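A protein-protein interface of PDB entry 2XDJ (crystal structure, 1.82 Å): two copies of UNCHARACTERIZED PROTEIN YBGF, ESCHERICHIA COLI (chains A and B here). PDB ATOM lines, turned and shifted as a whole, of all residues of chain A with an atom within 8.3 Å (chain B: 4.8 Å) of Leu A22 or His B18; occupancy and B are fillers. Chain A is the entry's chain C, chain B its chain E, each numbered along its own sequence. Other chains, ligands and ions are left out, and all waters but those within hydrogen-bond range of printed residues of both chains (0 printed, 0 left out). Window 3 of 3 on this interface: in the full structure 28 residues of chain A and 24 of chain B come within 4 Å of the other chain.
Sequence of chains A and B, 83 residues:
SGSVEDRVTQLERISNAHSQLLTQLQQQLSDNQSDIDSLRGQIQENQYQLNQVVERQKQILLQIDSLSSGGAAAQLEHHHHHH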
ATOM      1  N   LEU A  11       1.984 -21.539  19.317  1.00  0.00           N
ATOM      2  CA  LEU A  11       0.739 -20.910  18.854  1.00  0.00           C
ATOM      3  C   LEU A  11      -0.511 -21.646  19.289  1.00  0.00           C
ATOM      4  O   LEU A  11      -1.512 -21.000  19.584  1.00  0.00           O
ATOM      5  CB  LEU A  11       0.713 -20.804  17.332  1.00  0.00           C
ATOM      6  CG  LEU A  11       1.429 -19.595  16.728  1.00  0.00           C
ATOM      7  CD1 LEU A  11       2.723 -19.379  17.396  1.00  0.00           C
ATOM      8  CD2 LEU A  11       1.650 -19.858  15.230  1.00  0.00           C
ATOM      9  N   GLU A  12      -0.466 -22.980  19.258  1.00  0.00           N
ATOM     10  CA  GLU A  12      -1.607 -23.819  19.665  1.00  0.00           C
ATOM     11  C   GLU A  12      -1.830 -23.621  21.152  1.00  0.00           C
ATOM     12  O   GLU A  12      -2.972 -23.577  21.599  1.00  0.00           O
ATOM     13  CB  GLU A  12      -1.345 -25.306  19.398  1.00  0.00           C
ATOM     14  CG  GLU A  12      -1.226 -25.633  17.950  1.00  0.00           C
ATOM     15  CD  GLU A  12      -0.614 -27.042  17.696  1.00  0.00           C
ATOM     16  OE1 GLU A  12       0.311 -27.486  18.416  1.00  0.00           O
ATOM     17  OE2 GLU A  12      -1.060 -27.693  16.750  1.00  0.00           O
ATOM     18  N   ILE A  14      -1.008 -20.851  22.922  1.00  0.00           N
ATOM     19  CA  ILE A  14      -1.501 -19.490  23.168  1.00  0.00           C
ATOM     20  C   ILE A  14      -2.944 -19.431  22.625  1.00  0.00           C
ATOM     21  O   ILE A  14      -3.845 -18.766  23.193  1.00  0.00           O
ATOM     22  CB  ILE A  14      -0.637 -18.462  22.402  1.00  0.00           C
ATOM     23  CG1 ILE A  14       0.798 -18.341  22.980  1.00  0.00           C
ATOM     24  CG2 ILE A  14      -1.353 -17.090  22.284  1.00  0.00           C
ATOM     25  CD1 ILE A  14       0.901 -17.717  24.329  1.00  0.00           C
ATOM     26  N   SER A  15      -3.177 -20.136  21.529  1.00  0.00           N
ATOM     27  CA  SER A  15      -4.566 -20.198  20.981  1.00  0.00           C
ATOM     28  C   SER A  15      -5.544 -20.768  22.002  1.00  0.00           C
ATOM     29  O   SER A  15      -6.622 -20.227  22.204  1.00  0.00           O
ATOM     30  CB  SER A  15      -4.608 -20.975  19.663  1.00  0.00           C
ATOM     31  OG  SER A  15      -5.914 -20.932  19.083  1.00  0.00           O
ATOM     32  N   ASN A  16      -5.188 -21.877  22.636  1.00  0.00           N
ATOM     33  CA  ASN A  16      -5.999 -22.444  23.684  1.00  0.00           C
ATOM     34  C   ASN A  16      -6.282 -21.500  24.879  1.00  0.00           C
ATOM     35  O   ASN A  16      -7.449 -21.417  25.364  1.00  0.00           O
ATOM     36  CB  ASN A  16      -5.368 -23.774  24.144  1.00  0.00           C
ATOM     37  CG  ASN A  16      -6.317 -24.584  24.929  1.00  0.00           C
ATOM     38  OD1 ASN A  16      -7.489 -24.720  24.545  1.00  0.00           O
ATOM     39  ND2 ASN A  16      -5.861 -25.099  26.092  1.00  0.00           N
ATOM     40  N   ALA A  17      -5.263 -20.774  25.315  1.00  0.00           N
ATOM     41  CA  ALA A  17      -5.469 -19.779  26.372  1.00  0.00           C
ATOM     42  C   ALA A  17      -6.401 -18.689  25.891  1.00  0.00           C
ATOM     43  O   ALA A  17      -7.256 -18.276  26.633  1.00  0.00           O
ATOM     44  CB  ALA A  17      -4.174 -19.170  26.912  1.00  0.00           C
ATOM     45  N   HIS A  18      -6.259 -18.258  24.634  1.00  0.00           N
ATOM     46  CA  HIS A  18      -7.144 -17.196  24.092  1.00  0.00           C
ATOM     47  C   HIS A  18      -8.575 -17.694  23.993  1.00  0.00           C
ATOM     48  O   HIS A  18      -9.510 -16.946  24.355  1.00  0.00           O
ATOM     49  CB  HIS A  18      -6.639 -16.776  22.693  1.00  0.00           C
ATOM     50  CG  HIS A  18      -5.419 -15.910  22.715  1.00  0.00           C
ATOM     51  ND1 HIS A  18      -4.888 -15.377  21.557  1.00  0.00           N
ATOM     52  CD2 HIS A  18      -4.614 -15.507  23.717  1.00  0.00           C
ATOM     53  CE1 HIS A  18      -3.835 -14.637  21.858  1.00  0.00           C
ATOM     54  NE2 HIS A  18      -3.633 -14.712  23.159  1.00  0.00           N
ATOM     55  N   SER A  19      -8.770 -18.972  23.602  1.00  0.00           N
ATOM     56  CA  SER A  19     -10.109 -19.536  23.585  1.00  0.00           C
ATOM     57  C   SER A  19     -10.802 -19.493  24.963  1.00  0.00           C
ATOM     58  O   SER A  19     -11.980 -19.097  25.060  1.00  0.00           O
ATOM     59  CB  SER A  19     -10.138 -20.962  23.048  1.00  0.00           C
ATOM     60  OG  SER A  19      -9.816 -20.890  21.661  1.00  0.00           O
ATOM     61  N   GLN A  20     -10.088 -19.971  25.979  1.00  0.00           N
ATOM     62  CA  GLN A  20     -10.587 -19.990  27.339  1.00  0.00           C
ATOM     63  C   GLN A  20     -10.891 -18.601  27.821  1.00  0.00           C
ATOM     64  O   GLN A  20     -11.909 -18.407  28.464  1.00  0.00           O
ATOM     65  CB  GLN A  20      -9.599 -20.673  28.313  1.00  0.00           C
ATOM     66  CG  GLN A  20      -9.480 -22.187  28.010  1.00  0.00           C
ATOM     67  CD  GLN A  20     -10.874 -22.837  27.961  1.00  0.00           C
ATOM     68  OE1 GLN A  20     -11.570 -22.897  28.986  1.00  0.00           O
ATOM     69  NE2 GLN A  20     -11.300 -23.269  26.773  1.00  0.00           N
ATOM     70  N   LEU A  21     -10.007 -17.647  27.575  1.00  0.00           N
ATOM     71  CA  LEU A  21     -10.264 -16.302  28.081  1.00  0.00           C
ATOM     72  C   LEU A  21     -11.477 -15.690  27.334  1.00  0.00           C
ATOM     73  O   LEU A  21     -12.293 -15.004  27.942  1.00  0.00           O
ATOM     74  CB  LEU A  21      -9.008 -15.424  27.870  1.00  0.00           C
ATOM     75  CG  LEU A  21      -9.106 -13.936  28.274  1.00  0.00           C
ATOM     76  CD1 LEU A  21      -9.527 -13.763  29.751  1.00  0.00           C
ATOM     77  CD2 LEU A  21      -7.736 -13.231  28.031  1.00  0.00           C
ATOM     78  N   LEU A  22     -11.558 -15.897  26.011  1.00  0.00           N
ATOM     79  CA  LEU A  22     -12.662 -15.256  25.283  1.00  0.00           C
ATOM     80  C   LEU A  22     -14.011 -15.761  25.830  1.00  0.00           C
ATOM     81  O   LEU A  22     -14.920 -14.967  26.053  1.00  0.00           O
ATOM     82  CB  LEU A  22     -12.579 -15.564  23.782  1.00  0.00           C
ATOM     83  CG  LEU A  22     -11.560 -14.735  23.005  1.00  0.00           C
ATOM     84  CD1 LEU A  22     -11.256 -15.471  21.695  1.00  0.00           C
ATOM     85  CD2 LEU A  22     -12.186 -13.375  22.730  1.00  0.00           C
ATOM     86  N   THR A  23     -14.098 -17.054  26.139  1.00  0.00           N
ATOM     87  CA  THR A  23     -15.367 -17.575  26.671  1.00  0.00           C
ATOM     88  C   THR A  23     -15.624 -16.980  28.074  1.00  0.00           C
ATOM     89  O   THR A  23     -16.760 -16.640  28.420  1.00  0.00           O
ATOM     90  CB  THR A  23     -15.449 -19.139  26.694  1.00  0.00           C
ATOM     91  OG1 THR A  23     -16.668 -19.511  27.330  1.00  0.00           O
ATOM     92  CG2 THR A  23     -14.395 -19.712  27.613  1.00  0.00           C
ATOM     93  N   GLN A  24     -14.567 -16.817  28.888  1.00  0.00           N
ATOM     94  CA  GLN A  24     -14.768 -16.178  30.218  1.00  0.00           C
ATOM     95  C   GLN A  24     -15.252 -14.768  30.043  1.00  0.00           C
ATOM     96  O   GLN A  24     -16.188 -14.283  30.724  1.00  0.00           O
ATOM     97  CB  GLN A  24     -13.463 -16.176  31.010  1.00  0.00           C
ATOM     98  CG  GLN A  24     -12.863 -17.584  31.260  1.00  0.00           C
ATOM     99  CD  GLN A  24     -11.466 -17.553  31.866  1.00  0.00           C
ATOM    100  OE1 GLN A  24     -10.786 -16.518  31.859  1.00  0.00           O
ATOM    101  NE2 GLN A  24     -11.072 -18.662  32.469  1.00  0.00           N
ATOM    102  N   LEU A  25     -14.640 -14.037  29.128  1.00  0.00           N
ATOM    103  CA  LEU A  25     -15.044 -12.627  28.980  1.00  0.00           C
ATOM    104  C   LEU A  25     -16.494 -12.506  28.475  1.00  0.00           C
ATOM    105  O   LEU A  25     -17.227 -11.596  28.899  1.00  0.00           O
ATOM    106  CB  LEU A  25     -14.136 -11.896  27.994  1.00  0.00           C
ATOM    107  CG  LEU A  25     -12.655 -11.703  28.446  1.00  0.00           C
ATOM    108  CD1 LEU A  25     -11.821 -11.173  27.216  1.00  0.00           C
ATOM    109  CD2 LEU A  25     -12.442 -10.728  29.618  1.00  0.00           C
ATOM    110  N   GLN A  26     -16.869 -13.379  27.546  1.00  0.00           N
ATOM    111  CA  GLN A  26     -18.247 -13.380  27.044  1.00  0.00           C
ATOM    112  C   GLN A  26     -19.248 -13.564  28.200  1.00  0.00           C
ATOM    113  O   GLN A  26     -20.253 -12.838  28.284  1.00  0.00           O
ATOM    114  CB  GLN A  26     -18.444 -14.524  26.048  1.00  0.00           C
ATOM    115  CG  GLN A  26     -19.935 -14.615  25.547  1.00  0.00           C
ATOM    116  CD  GLN A  26     -20.382 -13.361  24.733  1.00  0.00           C
ATOM    117  OE1 GLN A  26     -20.187 -13.300  23.484  1.00  0.00           O
ATOM    118  NE2 GLN A  26     -20.941 -12.362  25.438  1.00  0.00           N
ATOM    119  N   GLN A  27     -18.955 -14.504  29.090  1.00  0.00           N
ATOM    120  CA  GLN A  27     -19.871 -14.724  30.219  1.00  0.00           C
ATOM    121  C   GLN A  27     -19.954 -13.517  31.104  1.00  0.00           C
ATOM    122  O   GLN A  27     -21.044 -13.130  31.609  1.00  0.00           O
ATOM    123  CB  GLN A  27     -19.368 -15.908  31.011  1.00  0.00           C
ATOM    124  CG  GLN A  27     -19.591 -17.254  30.238  1.00  0.00           C
ATOM    125  CD  GLN A  27     -21.088 -17.544  29.953  1.00  0.00           C
ATOM    126  OE1 GLN A  27     -21.935 -17.375  30.848  1.00  0.00           O
ATOM    127  NE2 GLN A  27     -21.417 -18.026  28.715  1.00  0.00           N
ATOM    128  N   GLN A  28     -18.784 -12.974  31.423  1.00  0.00           N
ATOM    129  CA  GLN A  28     -18.796 -11.727  32.268  1.00  0.00           C
ATOM    130  C   GLN A  28     -19.509 -10.511  31.621  1.00  0.00           C
ATOM    131  O   GLN A  28     -20.234  -9.794  32.312  1.00  0.00           O
ATOM    132  CB  GLN A  28     -17.343 -11.391  32.566  1.00  0.00           C
ATOM    133  CG  GLN A  28     -16.759 -12.380  33.490  1.00  0.00           C
ATOM    134  CD  GLN A  28     -15.341 -12.079  33.917  1.00  0.00           C
ATOM    135  OE1 GLN A  28     -15.035 -10.979  34.408  1.00  0.00           O
ATOM    136  NE2 GLN A  28     -14.466 -13.069  33.766  1.00  0.00           N
ATOM    137  N   LEU A  29     -19.327 -10.313  30.323  1.00  0.00           N
ATOM    138  CA  LEU A  29     -19.943  -9.182  29.593  1.00  0.00           C
ATOM    139  C   LEU A  29     -21.456  -9.297  29.627  1.00  0.00           C
ATOM    140  O   LEU A  29     -22.185  -8.308  29.862  1.00  0.00           O
ATOM    141  CB  LEU A  29     -19.372  -9.119  28.172  1.00  0.00           C
ATOM    142  CG  LEU A  29     -17.958  -8.446  28.096  1.00  0.00           C
ATOM    143  CD1 LEU A  29     -17.266  -8.765  26.793  1.00  0.00           C
ATOM    144  CD2 LEU A  29     -17.989  -6.924  28.277  1.00  0.00           C
ATOM    145  N   ILE B  14      -9.115 -21.213  13.687  1.00  0.00           N
ATOM    146  CA  ILE B  14      -9.323 -20.711  15.072  1.00  0.00           C
ATOM    147  C   ILE B  14      -8.988 -19.217  15.236  1.00  0.00           C
ATOM    148  O   ILE B  14      -9.760 -18.483  15.895  1.00  0.00           O
ATOM    149  CB  ILE B  14      -8.611 -21.596  16.132  1.00  0.00           C
ATOM    150  CG1 ILE B  14      -9.127 -23.033  16.075  1.00  0.00           C
ATOM    151  CG2 ILE B  14      -8.800 -21.066  17.548  1.00  0.00           C
ATOM    152  CD1 ILE B  14      -8.188 -24.061  16.779  1.00  0.00           C
ATOM    153  N   SER B  15      -7.885 -18.758  14.640  1.00  0.00           N
ATOM    154  CA  SER B  15      -7.484 -17.349  14.674  1.00  0.00           C
ATOM    155  C   SER B  15      -8.531 -16.365  14.052  1.00  0.00           C
ATOM    156  O   SER B  15      -8.855 -15.325  14.632  1.00  0.00           O
ATOM    157  CB  SER B  15      -6.127 -17.146  14.004  1.00  0.00           C
ATOM    158  OG  SER B  15      -5.716 -15.785  14.143  1.00  0.00           O
ATOM    159  N   ASN B  16      -9.060 -16.736  12.900  1.00  0.00           N
ATOM    160  CA  ASN B  16     -10.217 -16.067  12.321  1.00  0.00           C
ATOM    161  C   ASN B  16     -11.431 -16.058  13.282  1.00  0.00           C
ATOM    162  O   ASN B  16     -12.073 -15.015  13.440  1.00  0.00           O
ATOM    163  CB  ASN B  16     -10.607 -16.711  10.980  1.00  0.00           C
ATOM    164  CG  ASN B  16     -11.814 -16.029  10.331  1.00  0.00           C
ATOM    165  OD1 ASN B  16     -12.870 -16.654  10.103  1.00  0.00           O
ATOM    166  ND2 ASN B  16     -11.683 -14.735  10.058  1.00  0.00           N
ATOM    167  N   ALA B  17     -11.762 -17.212  13.870  1.00  0.00           N
ATOM    168  CA  ALA B  17     -12.857 -17.258  14.833  1.00  0.00           C
ATOM    169  C   ALA B  17     -12.609 -16.289  15.993  1.00  0.00           C
ATOM    170  O   ALA B  17     -13.559 -15.595  16.446  1.00  0.00           O
ATOM    171  CB  ALA B  17     -13.143 -18.634  15.338  1.00  0.00           C
ATOM    172  N   HIS B  18     -11.373 -16.240  16.495  1.00  0.00           N
ATOM    173  CA  HIS B  18     -11.068 -15.337  17.581  1.00  0.00           C
ATOM    174  C   HIS B  18     -11.179 -13.906  17.172  1.00  0.00           C
ATOM    175  O   HIS B  18     -11.664 -13.112  17.979  1.00  0.00           O
ATOM    176  CB  HIS B  18      -9.670 -15.561  18.133  1.00  0.00           C
ATOM    177  CG  HIS B  18      -9.535 -16.862  18.854  1.00  0.00           C
ATOM    178  ND1 HIS B  18      -8.316 -17.382  19.229  1.00  0.00           N
ATOM    179  CD2 HIS B  18     -10.469 -17.742  19.281  1.00  0.00           C
ATOM    180  CE1 HIS B  18      -8.511 -18.526  19.866  1.00  0.00           C
ATOM    181  NE2 HIS B  18      -9.807 -18.750  19.933  1.00  0.00           N
ATOM    182  N   SER B  19     -10.711 -13.536  15.950  1.00  0.00           N
ATOM    183  CA  SER B  19     -10.888 -12.119  15.497  1.00  0.00           C
ATOM    184  C   SER B  19     -12.355 -11.670  15.510  1.00  0.00           C
ATOM    185  O   SER B  19     -12.659 -10.570  15.968  1.00  0.00           O
ATOM    186  CB  SER B  19     -10.293 -11.847  14.106  1.00  0.00           C
ATOM    187  OG  SER B  19      -8.974 -12.331  14.009  1.00  0.00           O
ATOM    188  N   GLN B  20     -13.247 -12.528  15.026  1.00  0.00           N
ATOM    189  CA  GLN B  20     -14.685 -12.251  15.004  1.00  0.00           C
ATOM    190  C   GLN B  20     -15.206 -12.100  16.409  1.00  0.00           C
ATOM    191  O   GLN B  20     -15.960 -11.160  16.688  1.00  0.00           O
ATOM    192  CB  GLN B  20     -15.474 -13.379  14.391  1.00  0.00           C
ATOM    193  CG  GLN B  20     -15.076 -13.598  12.967  1.00  0.00           C
ATOM    194  CD  GLN B  20     -15.982 -14.507  12.195  1.00  0.00           C
ATOM    195  OE1 GLN B  20     -15.585 -14.990  11.143  1.00  0.00           O
ATOM    196  NE2 GLN B  20     -17.206 -14.723  12.677  1.00  0.00           N
ATOM    197  N   LEU B  21     -14.857 -13.045  17.287  1.00  0.00           N
ATOM    198  CA  LEU B  21     -15.377 -12.951  18.660  1.00  0.00           C
ATOM    199  C   LEU B  21     -14.854 -11.693  19.359  1.00  0.00           C
ATOM    200  O   LEU B  21     -15.596 -11.012  20.094  1.00  0.00           O
ATOM    201  CB  LEU B  21     -15.121 -14.262  19.441  1.00  0.00           C
ATOM    202  CG  LEU B  21     -15.795 -14.326  20.832  1.00  0.00           C
ATOM    203  CD1 LEU B  21     -17.270 -13.904  20.839  1.00  0.00           C
ATOM    204  CD2 LEU B  21     -15.551 -15.773  21.342  1.00  0.00           C
ATOM    205  N   LEU B  22     -13.590 -11.350  19.095  1.00  0.00           N
ATOM    206  CA  LEU B  22     -12.960 -10.197  19.710  1.00  0.00           C
ATOM    207  C   LEU B  22     -13.654  -8.927  19.375  1.00  0.00           C
ATOM    208  O   LEU B  22     -13.943  -8.107  20.265  1.00  0.00           O
ATOM    209  CB  LEU B  22     -11.534 -10.103  19.205  1.00  0.00           C
ATOM    210  CG  LEU B  22     -10.593 -10.820  20.137  1.00  0.00           C
ATOM    211  CD1 LEU B  22      -9.198 -10.819  19.443  1.00  0.00           C
ATOM    212  CD2 LEU B  22     -10.492 -10.120  21.520  1.00  0.00           C
ATOM    213  N   LEU B  25     -17.016  -8.934  21.276  1.00  0.00           N
ATOM    214  CA  LEU B  25     -16.883  -8.584  22.725  1.00  0.00           C
ATOM    215  C   LEU B  25     -16.491  -7.096  22.929  1.00  0.00           C
ATOM    216  O   LEU B  25     -16.948  -6.424  23.885  1.00  0.00           O
ATOM    217  CB  LEU B  25     -15.868  -9.489  23.404  1.00  0.00           C
ATOM    218  CG  LEU B  25     -16.264 -10.972  23.357  1.00  0.00           C
ATOM    219  CD1 LEU B  25     -15.228 -11.709  24.290  1.00  0.00           C
ATOM    220  CD2 LEU B  25     -17.687 -11.204  23.855  1.00  0.00           C
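OG of Ser A19 sits at hydrogen-bond distance from NE2 of His B18 (2.8 Å).
The backbone carbonyl oxygen (O) of Ser A15 is in hydrogen-bond range of the side-chain hydroxyl (OG) of Ser A19 (3.3 Å).
Ile B14 touches Ser A15 (CG2 to OG, 3.3 Å). His B18 touches Ser A15. Leu A22 touches His B18 (CD1 to CD2, 3.4 Å). Leu A22 touches Leu B21 (CB to CD2, 3.9 Å). Leu A22 touches Leu B22. Leu A22 touches Leu B25. Leu B25 touches Leu A25. Gln A26 touches Leu B21 (OE1 to CD1, 3.98 Å). Gln A26 touches Leu B25 (OE1 to CD2, 3.3 Å). CD1 of Leu A29 touches CB of Leu B25, at 3.7 Å.
Of the printed residues of chain B, Gln A26 touches Leu B21 and Leu B25. Of the printed residues of chain B, Leu A29 touches Leu B25 (3.7 Å). Printed residues of chain A within 4 Å of Ile B14: Ser A15. No residue of chain A comes within 4 Å of Ser B19. The nearest printed residue of chain B that does not touch Ser A19 is Ile B14 (4.2 Å).
Hydrophobic or aromatic side chains of chain A within 4 Å of the printed part of chain B: His A18, Leu A22, Leu A25 and Leu A29. Of the 10 printed residues of chain B, 5 touch a printed residue of chain A. Hydrophobic or aromatic side chains of chain B that line the printed part of chain A: Ile B14, His B18, Leu B21, Leu B22 and Leu B25. Along chain B the printed residues that touch a printed residue of chain A span positions 14 to 25.
Ser A15 touches Ile B14, but with the chains exchanged Ile A14 does not touch Ser B15 (9.3 Å). Leu A22 touches Leu B21, but with the chains exchanged Leu A21 does not touch Leu B22 (7.7 Å). Leu A22 touches Leu B25, but with the chains exchanged Leu A25 does not touch Leu B22 (5.9 Å). Leu A25 touches its own counterpart, Leu B25.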
